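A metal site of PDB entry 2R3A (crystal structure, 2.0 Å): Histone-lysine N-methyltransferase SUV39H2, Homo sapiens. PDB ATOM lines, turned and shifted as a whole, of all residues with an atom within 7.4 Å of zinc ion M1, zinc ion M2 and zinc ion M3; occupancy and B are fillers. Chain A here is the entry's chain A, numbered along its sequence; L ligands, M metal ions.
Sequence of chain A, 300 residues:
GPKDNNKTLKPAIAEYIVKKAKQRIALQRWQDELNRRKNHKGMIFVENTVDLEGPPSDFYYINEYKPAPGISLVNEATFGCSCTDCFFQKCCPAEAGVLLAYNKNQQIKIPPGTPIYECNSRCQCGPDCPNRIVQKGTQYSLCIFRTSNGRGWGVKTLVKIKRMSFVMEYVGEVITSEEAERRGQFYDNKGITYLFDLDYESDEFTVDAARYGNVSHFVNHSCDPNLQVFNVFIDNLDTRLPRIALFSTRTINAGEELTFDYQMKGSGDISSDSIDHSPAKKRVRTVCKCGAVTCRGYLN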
ATOM      1  N   PHE A  79     -26.859  23.660 -21.575  1.00  0.00           N
ATOM      2  CA  PHE A  79     -25.943  24.083 -22.627  1.00  0.00           C
ATOM      3  C   PHE A  79     -24.529  23.601 -22.253  1.00  0.00           C
ATOM      4  O   PHE A  79     -24.142  23.572 -21.067  1.00  0.00           O
ATOM      5  CB  PHE A  79     -25.932  25.616 -22.800  1.00  0.00           C
ATOM      6  CG  PHE A  79     -27.304  26.239 -22.996  1.00  0.00           C
ATOM      7  CD1 PHE A  79     -27.927  26.204 -24.239  1.00  0.00           C
ATOM      8  CD2 PHE A  79     -27.941  26.913 -21.947  1.00  0.00           C
ATOM      9  CE1 PHE A  79     -29.178  26.811 -24.433  1.00  0.00           C
ATOM     10  CE2 PHE A  79     -29.186  27.518 -22.149  1.00  0.00           C
ATOM     11  CZ  PHE A  79     -29.797  27.471 -23.393  1.00  0.00           C
ATOM     12  N   GLY A  80     -23.773  23.208 -23.269  1.00  0.00           N
ATOM     13  CA  GLY A  80     -22.377  22.915 -23.091  1.00  0.00           C
ATOM     14  C   GLY A  80     -21.567  23.821 -23.984  1.00  0.00           C
ATOM     15  O   GLY A  80     -22.104  24.717 -24.641  1.00  0.00           O
ATOM     16  N   CYS A  81     -20.261  23.554 -23.987  1.00  0.00           N
ATOM     17  CA  CYS A  81     -19.290  24.209 -24.855  1.00  0.00           C
ATOM     18  C   CYS A  81     -19.244  23.496 -26.218  1.00  0.00           C
ATOM     19  O   CYS A  81     -19.811  22.415 -26.361  1.00  0.00           O
ATOM     20  CB  CYS A  81     -17.909  24.103 -24.176  1.00  0.00           C
ATOM     21  SG  CYS A  81     -17.218  22.404 -24.119  1.00  0.00           S
ATOM     22  N   SER A  82     -18.517  24.073 -27.183  1.00  0.00           N
ATOM     23  CA  SER A  82     -18.354  23.489 -28.524  1.00  0.00           C
ATOM     24  C   SER A  82     -16.909  23.317 -28.966  1.00  0.00           C
ATOM     25  O   SER A  82     -16.667  23.036 -30.182  1.00  0.00           O
ATOM     26  CB  SER A  82     -19.070  24.321 -29.606  1.00  0.00           C
ATOM     27  OG  SER A  82     -20.028  25.185 -29.069  1.00  0.00           O
ATOM     28  N   CYS A  83     -15.970  23.506 -28.023  1.00  0.00           N
ATOM     29  CA  CYS A  83     -14.552  23.268 -28.212  1.00  0.00           C
ATOM     30  C   CYS A  83     -14.242  21.979 -28.922  1.00  0.00           C
ATOM     31  O   CYS A  83     -14.871  20.932 -28.669  1.00  0.00           O
ATOM     32  CB  CYS A  83     -13.799  23.294 -26.876  1.00  0.00           C
ATOM     33  SG  CYS A  83     -14.383  24.519 -25.692  1.00  0.00           S
ATOM     34  N   THR A  84     -13.264  22.073 -29.819  1.00  0.00           N
ATOM     35  CA  THR A  84     -12.563  20.902 -30.322  1.00  0.00           C
ATOM     36  C   THR A  84     -11.304  20.646 -29.456  1.00  0.00           C
ATOM     37  O   THR A  84     -10.738  19.556 -29.474  1.00  0.00           O
ATOM     38  CB  THR A  84     -12.142  21.063 -31.777  1.00  0.00           C
ATOM     39  OG1 THR A  84     -11.491  22.327 -31.954  1.00  0.00           O
ATOM     40  CG2 THR A  84     -13.354  20.959 -32.743  1.00  0.00           C
ATOM     41  N   ASP A  85     -10.890  21.668 -28.715  1.00  0.00           N
ATOM     42  CA  ASP A  85      -9.814  21.569 -27.734  1.00  0.00           C
ATOM     43  C   ASP A  85     -10.238  22.333 -26.476  1.00  0.00           C
ATOM     44  O   ASP A  85     -10.003  23.538 -26.356  1.00  0.00           O
ATOM     45  CB  ASP A  85      -8.517  22.144 -28.307  1.00  0.00           C
ATOM     46  CG  ASP A  85      -7.285  21.789 -27.465  1.00  0.00           C
ATOM     47  OD1 ASP A  85      -7.415  21.339 -26.322  1.00  0.00           O
ATOM     48  OD2 ASP A  85      -6.161  21.977 -27.991  1.00  0.00           O
ATOM     49  N   CYS A  86     -10.910  21.634 -25.548  1.00  0.00           N
ATOM     50  CA  CYS A  86     -11.403  22.285 -24.306  1.00  0.00           C
ATOM     51  C   CYS A  86     -10.281  22.789 -23.415  1.00  0.00           C
ATOM     52  O   CYS A  86     -10.481  23.697 -22.606  1.00  0.00           O
ATOM     53  CB  CYS A  86     -12.258  21.325 -23.510  1.00  0.00           C
ATOM     54  SG  CYS A  86     -13.833  21.035 -24.266  1.00  0.00           S
ATOM     55  N   PHE A  87      -9.101  22.204 -23.548  1.00  0.00           N
ATOM     56  CA  PHE A  87      -7.953  22.664 -22.766  1.00  0.00           C
ATOM     57  C   PHE A  87      -7.499  24.111 -23.131  1.00  0.00           C
ATOM     58  O   PHE A  87      -7.059  24.877 -22.263  1.00  0.00           O
ATOM     59  CB  PHE A  87      -6.790  21.660 -22.848  1.00  0.00           C
ATOM     60  CG  PHE A  87      -5.721  21.910 -21.824  1.00  0.00           C
ATOM     61  CD1 PHE A  87      -5.896  21.493 -20.495  1.00  0.00           C
ATOM     62  CD2 PHE A  87      -4.554  22.615 -22.153  1.00  0.00           C
ATOM     63  CE1 PHE A  87      -4.911  21.769 -19.523  1.00  0.00           C
ATOM     64  CE2 PHE A  87      -3.565  22.881 -21.188  1.00  0.00           C
ATOM     65  CZ  PHE A  87      -3.748  22.464 -19.865  1.00  0.00           C
ATOM     66  N   GLN A  89      -9.346  26.301 -25.712  1.00  0.00           N
ATOM     67  CA  GLN A  89     -10.419  27.193 -26.191  1.00  0.00           C
ATOM     68  C   GLN A  89     -11.271  27.713 -25.031  1.00  0.00           C
ATOM     69  O   GLN A  89     -11.103  27.274 -23.889  1.00  0.00           O
ATOM     70  CB  GLN A  89     -11.268  26.475 -27.259  1.00  0.00           C
ATOM     71  CG  GLN A  89     -10.455  26.125 -28.502  1.00  0.00           C
ATOM     72  CD  GLN A  89     -11.291  25.486 -29.562  1.00  0.00           C
ATOM     73  OE1 GLN A  89     -12.096  24.596 -29.289  1.00  0.00           O
ATOM     74  NE2 GLN A  89     -11.094  25.936 -30.832  1.00  0.00           N
ATOM     75  N   LYS A  90     -12.161  28.649 -25.315  1.00  0.00           N
ATOM     76  CA  LYS A  90     -13.057  29.185 -24.263  1.00  0.00           C
ATOM     77  C   LYS A  90     -14.139  28.149 -23.999  1.00  0.00           C
ATOM     78  O   LYS A  90     -14.911  27.809 -24.895  1.00  0.00           O
ATOM     79  CB  LYS A  90     -13.695  30.510 -24.686  1.00  0.00           C
ATOM     80  CG  LYS A  90     -12.862  31.738 -24.418  1.00  0.00           C
ATOM     81  CD  LYS A  90     -13.518  32.980 -25.012  1.00  0.00           C
ATOM     82  CE  LYS A  90     -12.716  33.527 -26.204  1.00  0.00           C
ATOM     83  NZ  LYS A  90     -11.591  34.362 -25.694  1.00  0.00           N
ATOM     84  N   CYS A  91     -14.180  27.633 -22.780  1.00  0.00           N
ATOM     85  CA  CYS A  91     -14.868  26.406 -22.462  1.00  0.00           C
ATOM     86  C   CYS A  91     -15.840  26.640 -21.285  1.00  0.00           C
ATOM     87  O   CYS A  91     -16.086  27.780 -20.900  1.00  0.00           O
ATOM     88  CB  CYS A  91     -13.806  25.360 -22.136  1.00  0.00           C
ATOM     89  SG  CYS A  91     -14.361  23.722 -21.684  1.00  0.00           S
ATOM     90  N   CYS A  92     -16.392  25.556 -20.747  1.00  0.00           N
ATOM     91  CA  CYS A  92     -17.355  25.680 -19.643  1.00  0.00           C
ATOM     92  C   CYS A  92     -16.929  26.528 -18.441  1.00  0.00           C
ATOM     93  O   CYS A  92     -17.720  27.365 -17.966  1.00  0.00           O
ATOM     94  CB  CYS A  92     -17.859  24.298 -19.203  1.00  0.00           C
ATOM     95  SG  CYS A  92     -18.793  23.367 -20.515  1.00  0.00           S
ATOM     96  N   PRO A  93     -15.690  26.316 -17.919  1.00  0.00           N
ATOM     97  CA  PRO A  93     -15.329  27.196 -16.793  1.00  0.00           C
ATOM     98  C   PRO A  93     -15.339  28.695 -17.162  1.00  0.00           C
ATOM     99  O   PRO A  93     -15.856  29.510 -16.401  1.00  0.00           O
ATOM    100  CB  PRO A  93     -13.899  26.736 -16.388  1.00  0.00           C
ATOM    101  CG  PRO A  93     -13.649  25.476 -17.096  1.00  0.00           C
ATOM    102  CD  PRO A  93     -14.600  25.400 -18.267  1.00  0.00           C
ATOM    103  N   TYR A 117     -16.161  23.529 -12.757  1.00  0.00           N
ATOM    104  CA  TYR A 117     -17.211  23.409 -13.779  1.00  0.00           C
ATOM    105  C   TYR A 117     -16.633  22.499 -14.839  1.00  0.00           C
ATOM    106  O   TYR A 117     -15.774  22.911 -15.643  1.00  0.00           O
ATOM    107  CB  TYR A 117     -17.618  24.778 -14.381  1.00  0.00           C
ATOM    108  CG  TYR A 117     -18.527  25.577 -13.474  1.00  0.00           C
ATOM    109  CD1 TYR A 117     -19.927  25.510 -13.613  1.00  0.00           C
ATOM    110  CD2 TYR A 117     -18.001  26.393 -12.480  1.00  0.00           C
ATOM    111  CE1 TYR A 117     -20.745  26.210 -12.772  1.00  0.00           C
ATOM    112  CE2 TYR A 117     -18.827  27.107 -11.610  1.00  0.00           C
ATOM    113  CZ  TYR A 117     -20.199  27.014 -11.774  1.00  0.00           C
ATOM    114  OH  TYR A 117     -21.060  27.738 -10.956  1.00  0.00           O
ATOM    115  N   GLU A 118     -17.039  21.240 -14.811  1.00  0.00           N
ATOM    116  CA  GLU A 118     -16.560  20.259 -15.791  1.00  0.00           C
ATOM    117  C   GLU A 118     -17.468  20.303 -17.027  1.00  0.00           C
ATOM    118  O   GLU A 118     -18.597  20.825 -16.970  1.00  0.00           O
ATOM    119  CB  GLU A 118     -16.577  18.820 -15.243  1.00  0.00           C
ATOM    120  CG  GLU A 118     -15.685  18.617 -14.001  1.00  0.00           C
ATOM    121  CD  GLU A 118     -15.207  17.188 -13.846  1.00  0.00           C
ATOM    122  OE1 GLU A 118     -15.835  16.236 -14.354  1.00  0.00           O
ATOM    123  OE2 GLU A 118     -14.163  16.984 -13.190  1.00  0.00           O
ATOM    124  N   CYS A 119     -17.006  19.729 -18.132  1.00  0.00           N
ATOM    125  CA  CYS A 119     -17.849  19.580 -19.288  1.00  0.00           C
ATOM    126  C   CYS A 119     -18.914  18.514 -18.981  1.00  0.00           C
ATOM    127  O   CYS A 119     -18.745  17.690 -18.065  1.00  0.00           O
ATOM    128  CB  CYS A 119     -17.018  19.179 -20.509  1.00  0.00           C
ATOM    129  SG  CYS A 119     -15.937  20.474 -21.056  1.00  0.00           S
ATOM    130  N   ASN A 120     -20.008  18.544 -19.739  1.00  0.00           N
ATOM    131  CA  ASN A 120     -21.210  17.819 -19.345  1.00  0.00           C
ATOM    132  C   ASN A 120     -21.827  17.117 -20.560  1.00  0.00           C
ATOM    133  O   ASN A 120     -21.179  17.078 -21.630  1.00  0.00           O
ATOM    134  CB  ASN A 120     -22.179  18.761 -18.630  1.00  0.00           C
ATOM    135  CG  ASN A 120     -22.646  19.932 -19.511  1.00  0.00           C
ATOM    136  OD1 ASN A 120     -23.302  19.738 -20.537  1.00  0.00           O
ATOM    137  ND2 ASN A 120     -22.322  21.139 -19.105  1.00  0.00           N
ATOM    138  N   ARG A 122     -24.082  17.858 -22.497  1.00  0.00           N
ATOM    139  CA  ARG A 122     -24.415  18.772 -23.570  1.00  0.00           C
ATOM    140  C   ARG A 122     -23.212  19.303 -24.326  1.00  0.00           C
ATOM    141  O   ARG A 122     -23.386  19.893 -25.376  1.00  0.00           O
ATOM    142  CB  ARG A 122     -25.272  19.936 -23.040  1.00  0.00           C
ATOM    143  N   CYS A 123     -21.980  19.143 -23.806  1.00  0.00           N
ATOM    144  CA  CYS A 123     -20.790  19.608 -24.533  1.00  0.00           C
ATOM    145  C   CYS A 123     -20.501  18.685 -25.722  1.00  0.00           C
ATOM    146  O   CYS A 123     -20.860  17.501 -25.686  1.00  0.00           O
ATOM    147  CB  CYS A 123     -19.562  19.624 -23.614  1.00  0.00           C
ATOM    148  SG  CYS A 123     -19.806  20.646 -22.151  1.00  0.00           S
ATOM    149  N   GLN A 124     -19.818  19.214 -26.735  1.00  0.00           N
ATOM    150  CA  GLN A 124     -19.464  18.444 -27.931  1.00  0.00           C
ATOM    151  C   GLN A 124     -18.357  17.433 -27.715  1.00  0.00           C
ATOM    152  O   GLN A 124     -18.249  16.440 -28.474  1.00  0.00           O
ATOM    153  CB  GLN A 124     -19.057  19.361 -29.087  1.00  0.00           C
ATOM    154  CG  GLN A 124     -20.178  20.247 -29.723  1.00  0.00           C
ATOM    155  CD  GLN A 124     -21.354  19.436 -30.262  1.00  0.00           C
ATOM    156  OE1 GLN A 124     -21.205  18.569 -31.151  1.00  0.00           O
ATOM    157  NE2 GLN A 124     -22.533  19.701 -29.734  1.00  0.00           N
ATOM    158  N   CYS A 125     -17.496  17.709 -26.707  1.00  0.00           N
ATOM    159  CA  CYS A 125     -16.298  16.913 -26.442  1.00  0.00           C
ATOM    160  C   CYS A 125     -16.624  15.523 -25.923  1.00  0.00           C
ATOM    161  O   CYS A 125     -17.653  15.303 -25.275  1.00  0.00           O
ATOM    162  CB  CYS A 125     -15.394  17.629 -25.434  1.00  0.00           C
ATOM    163  SG  CYS A 125     -16.258  17.995 -23.846  1.00  0.00           S
ATOM    164  N   GLY A 126     -15.719  14.598 -26.190  1.00  0.00           N
ATOM    165  CA  GLY A 126     -15.853  13.217 -25.747  1.00  0.00           C
ATOM    166  C   GLY A 126     -15.223  13.000 -24.366  1.00  0.00           C
ATOM    167  O   GLY A 126     -14.769  13.947 -23.721  1.00  0.00           O
ATOM    168  N   ASP A 128     -12.430  11.816 -23.182  1.00  0.00           N
ATOM    169  CA  ASP A 128     -11.048  12.123 -22.876  1.00  0.00           C
ATOM    170  C   ASP A 128     -10.746  13.631 -22.888  1.00  0.00           C
ATOM    171  O   ASP A 128      -9.586  14.054 -22.860  1.00  0.00           O
ATOM    172  CB  ASP A 128     -10.114  11.234 -23.724  1.00  0.00           C
ATOM    173  CG  ASP A 128     -10.400   9.698 -23.547  1.00  0.00           C
ATOM    174  OD1 ASP A 128     -10.797   9.232 -22.429  1.00  0.00           O
ATOM    175  OD2 ASP A 128     -10.215   8.948 -24.543  1.00  0.00           O
ATOM    176  N   CYS A 129     -11.798  14.454 -22.856  1.00  0.00           N
ATOM    177  CA  CYS A 129     -11.668  15.872 -22.539  1.00  0.00           C
ATOM    178  C   CYS A 129     -10.934  16.075 -21.174  1.00  0.00           C
ATOM    179  O   CYS A 129     -11.288  15.462 -20.147  1.00  0.00           O
ATOM    180  CB  CYS A 129     -13.030  16.554 -22.503  1.00  0.00           C
ATOM    181  SG  CYS A 129     -12.980  18.244 -21.859  1.00  0.00           S
ATOM    182  N   PRO A 130      -9.900  16.939 -21.168  1.00  0.00           N
ATOM    183  CA  PRO A 130      -9.133  17.144 -19.953  1.00  0.00           C
ATOM    184  C   PRO A 130      -9.998  17.829 -18.895  1.00  0.00           C
ATOM    185  O   PRO A 130      -9.557  17.980 -17.765  1.00  0.00           O
ATOM    186  CB  PRO A 130      -8.009  18.088 -20.406  1.00  0.00           C
ATOM    187  CG  PRO A 130      -8.624  18.830 -21.549  1.00  0.00           C
ATOM    188  CD  PRO A 130      -9.387  17.786 -22.273  1.00  0.00           C
ATOM    189  N   ASN A 131     -11.202  18.291 -19.288  1.00  0.00           N
ATOM    190  CA  ASN A 131     -12.152  18.879 -18.310  1.00  0.00           C
ATOM    191  C   ASN A 131     -13.238  17.890 -17.847  1.00  0.00           C
ATOM    192  O   ASN A 131     -14.311  18.276 -17.402  1.00  0.00           O
ATOM    193  CB  ASN A 131     -12.671  20.243 -18.792  1.00  0.00           C
ATOM    194  CG  ASN A 131     -13.445  21.029 -17.713  1.00  0.00           C
ATOM    195  OD1 ASN A 131     -14.344  21.819 -18.050  1.00  0.00           O
ATOM    196  ND2 ASN A 131     -13.075  20.866 -16.464  1.00  0.00           N
ATOM    197  N   ARG A 132     -12.948  16.600 -17.913  1.00  0.00           N
ATOM    198  CA  ARG A 132     -13.901  15.587 -17.413  1.00  0.00           C
ATOM    199  C   ARG A 132     -13.137  14.632 -16.496  1.00  0.00           C
ATOM    200  O   ARG A 132     -12.615  13.621 -16.958  1.00  0.00           O
ATOM    201  CB  ARG A 132     -14.509  14.816 -18.597  1.00  0.00           C
ATOM    202  CG  ARG A 132     -15.441  15.639 -19.534  1.00  0.00           C
ATOM    203  CD  ARG A 132     -15.824  14.773 -20.764  1.00  0.00           C
ATOM    204  NE  ARG A 132     -16.727  15.428 -21.724  1.00  0.00           N
ATOM    205  CZ  ARG A 132     -18.036  15.566 -21.576  1.00  0.00           C
ATOM    206  NH1 ARG A 132     -18.660  15.118 -20.486  1.00  0.00           N
ATOM    207  NH2 ARG A 132     -18.748  16.145 -22.535  1.00  0.00           N
HETATM  208  N1  LIG L   1      -9.492  16.456 -25.949  1.00  0.00           N
HETATM  209  C1  LIG L   1     -10.994  16.545 -25.966  1.00  0.00           C
HETATM  210  C2  LIG L   1     -11.720  15.438 -26.763  1.00  0.00           C
HETATM  211  O1  LIG L   1     -11.303  14.252 -26.721  1.00  0.00           O
HETATM  212  C3  LIG L   1     -11.441  17.967 -26.370  1.00  0.00           C
HETATM  213  O2  LIG L   1     -10.816  18.929 -25.532  1.00  0.00           O
HETATM  214  O3  LIG L   1     -12.761  15.682 -27.436  1.00  0.00           O
HETATM  215 ZN    ZN M   1     -14.902  22.981 -23.930  1.00  0.00          ZN
HETATM  216 ZN    ZN M   2     -17.796  21.829 -21.857  1.00  0.00          ZN
HETATM  217 ZN    ZN M   3     -14.807  19.427 -22.840  1.00  0.00          ZN
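Within 4 Å of zinc ion M3: Cys 86, Cys 119, Cys 125 and Cys 129. The nearest printed residue that does not touch zinc ion M3 is Cys 81 (4.04 Å).
Zinc ion M3 is bound by SG of Cys 125 (2.3 Å), SG of Cys 119 (2.4 Å), SG of Cys 86 (2.4 Å) and SG of Cys 129 (2.4 Å).
Zinc ion M2 is bound by SG of Cys 92 (2.3 Å), SG of Cys 123 (2.4 Å), SG of Cys 81 (2.4 Å) and SG of Cys 119 (2.4 Å).
SG of Cys 129 sits close to N of Asn 131, at 3.1 Å. SG of Cys 123 lies close to N of Asn 120, 3.2 Å away. The side-chain sulfur (SG) of Cys 83 lies close to the backbone carbonyl oxygen (O) of Lys 90 (3.4 Å). O of Cys 125 sits at hydrogen-bond distance from NH2 of Arg 132 (3.1 Å). The backbone NH of Cys 119 sits at hydrogen-bond distance from the backbone carbonyl oxygen of Asn 131, at 3.1 Å. O of Cys 81 sits at hydrogen-bond distance from N of Gln 124, at 3.2 Å.
N of Gly 126 is in hydrogen-bond range of O3 of the ligand (3.4 Å). The backbone NH of Cys 86 is in hydrogen-bond range of an oxygen (O2) of the ligand (2.7 Å).
Zinc ion M1 is bound by the side-chain sulfur (SG) of Cys 86 (2.2 Å), the side-chain sulfur (SG) of Cys 81 (2.4 Å), the side-chain sulfur (SG) of Cys 83 (2.4 Å) and the side-chain sulfur (SG) of Cys 91 (2.4 Å). Zinc ion M1 has four donor atoms within binding distance.
Along chain A the residues within 4 Å of zinc ion M1 span positions 81 to 119. The nearest printed residue that does not touch zinc ion M1 is Cys 92 (4.4 Å).
Five residues have an atom within 4 Å of zinc ion M2: Cys 81, Cys 91, Cys 92, Cys 119 and Cys 123. The nearest printed residue that does not touch zinc ion M2 is Asn 120 (4.5 Å).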
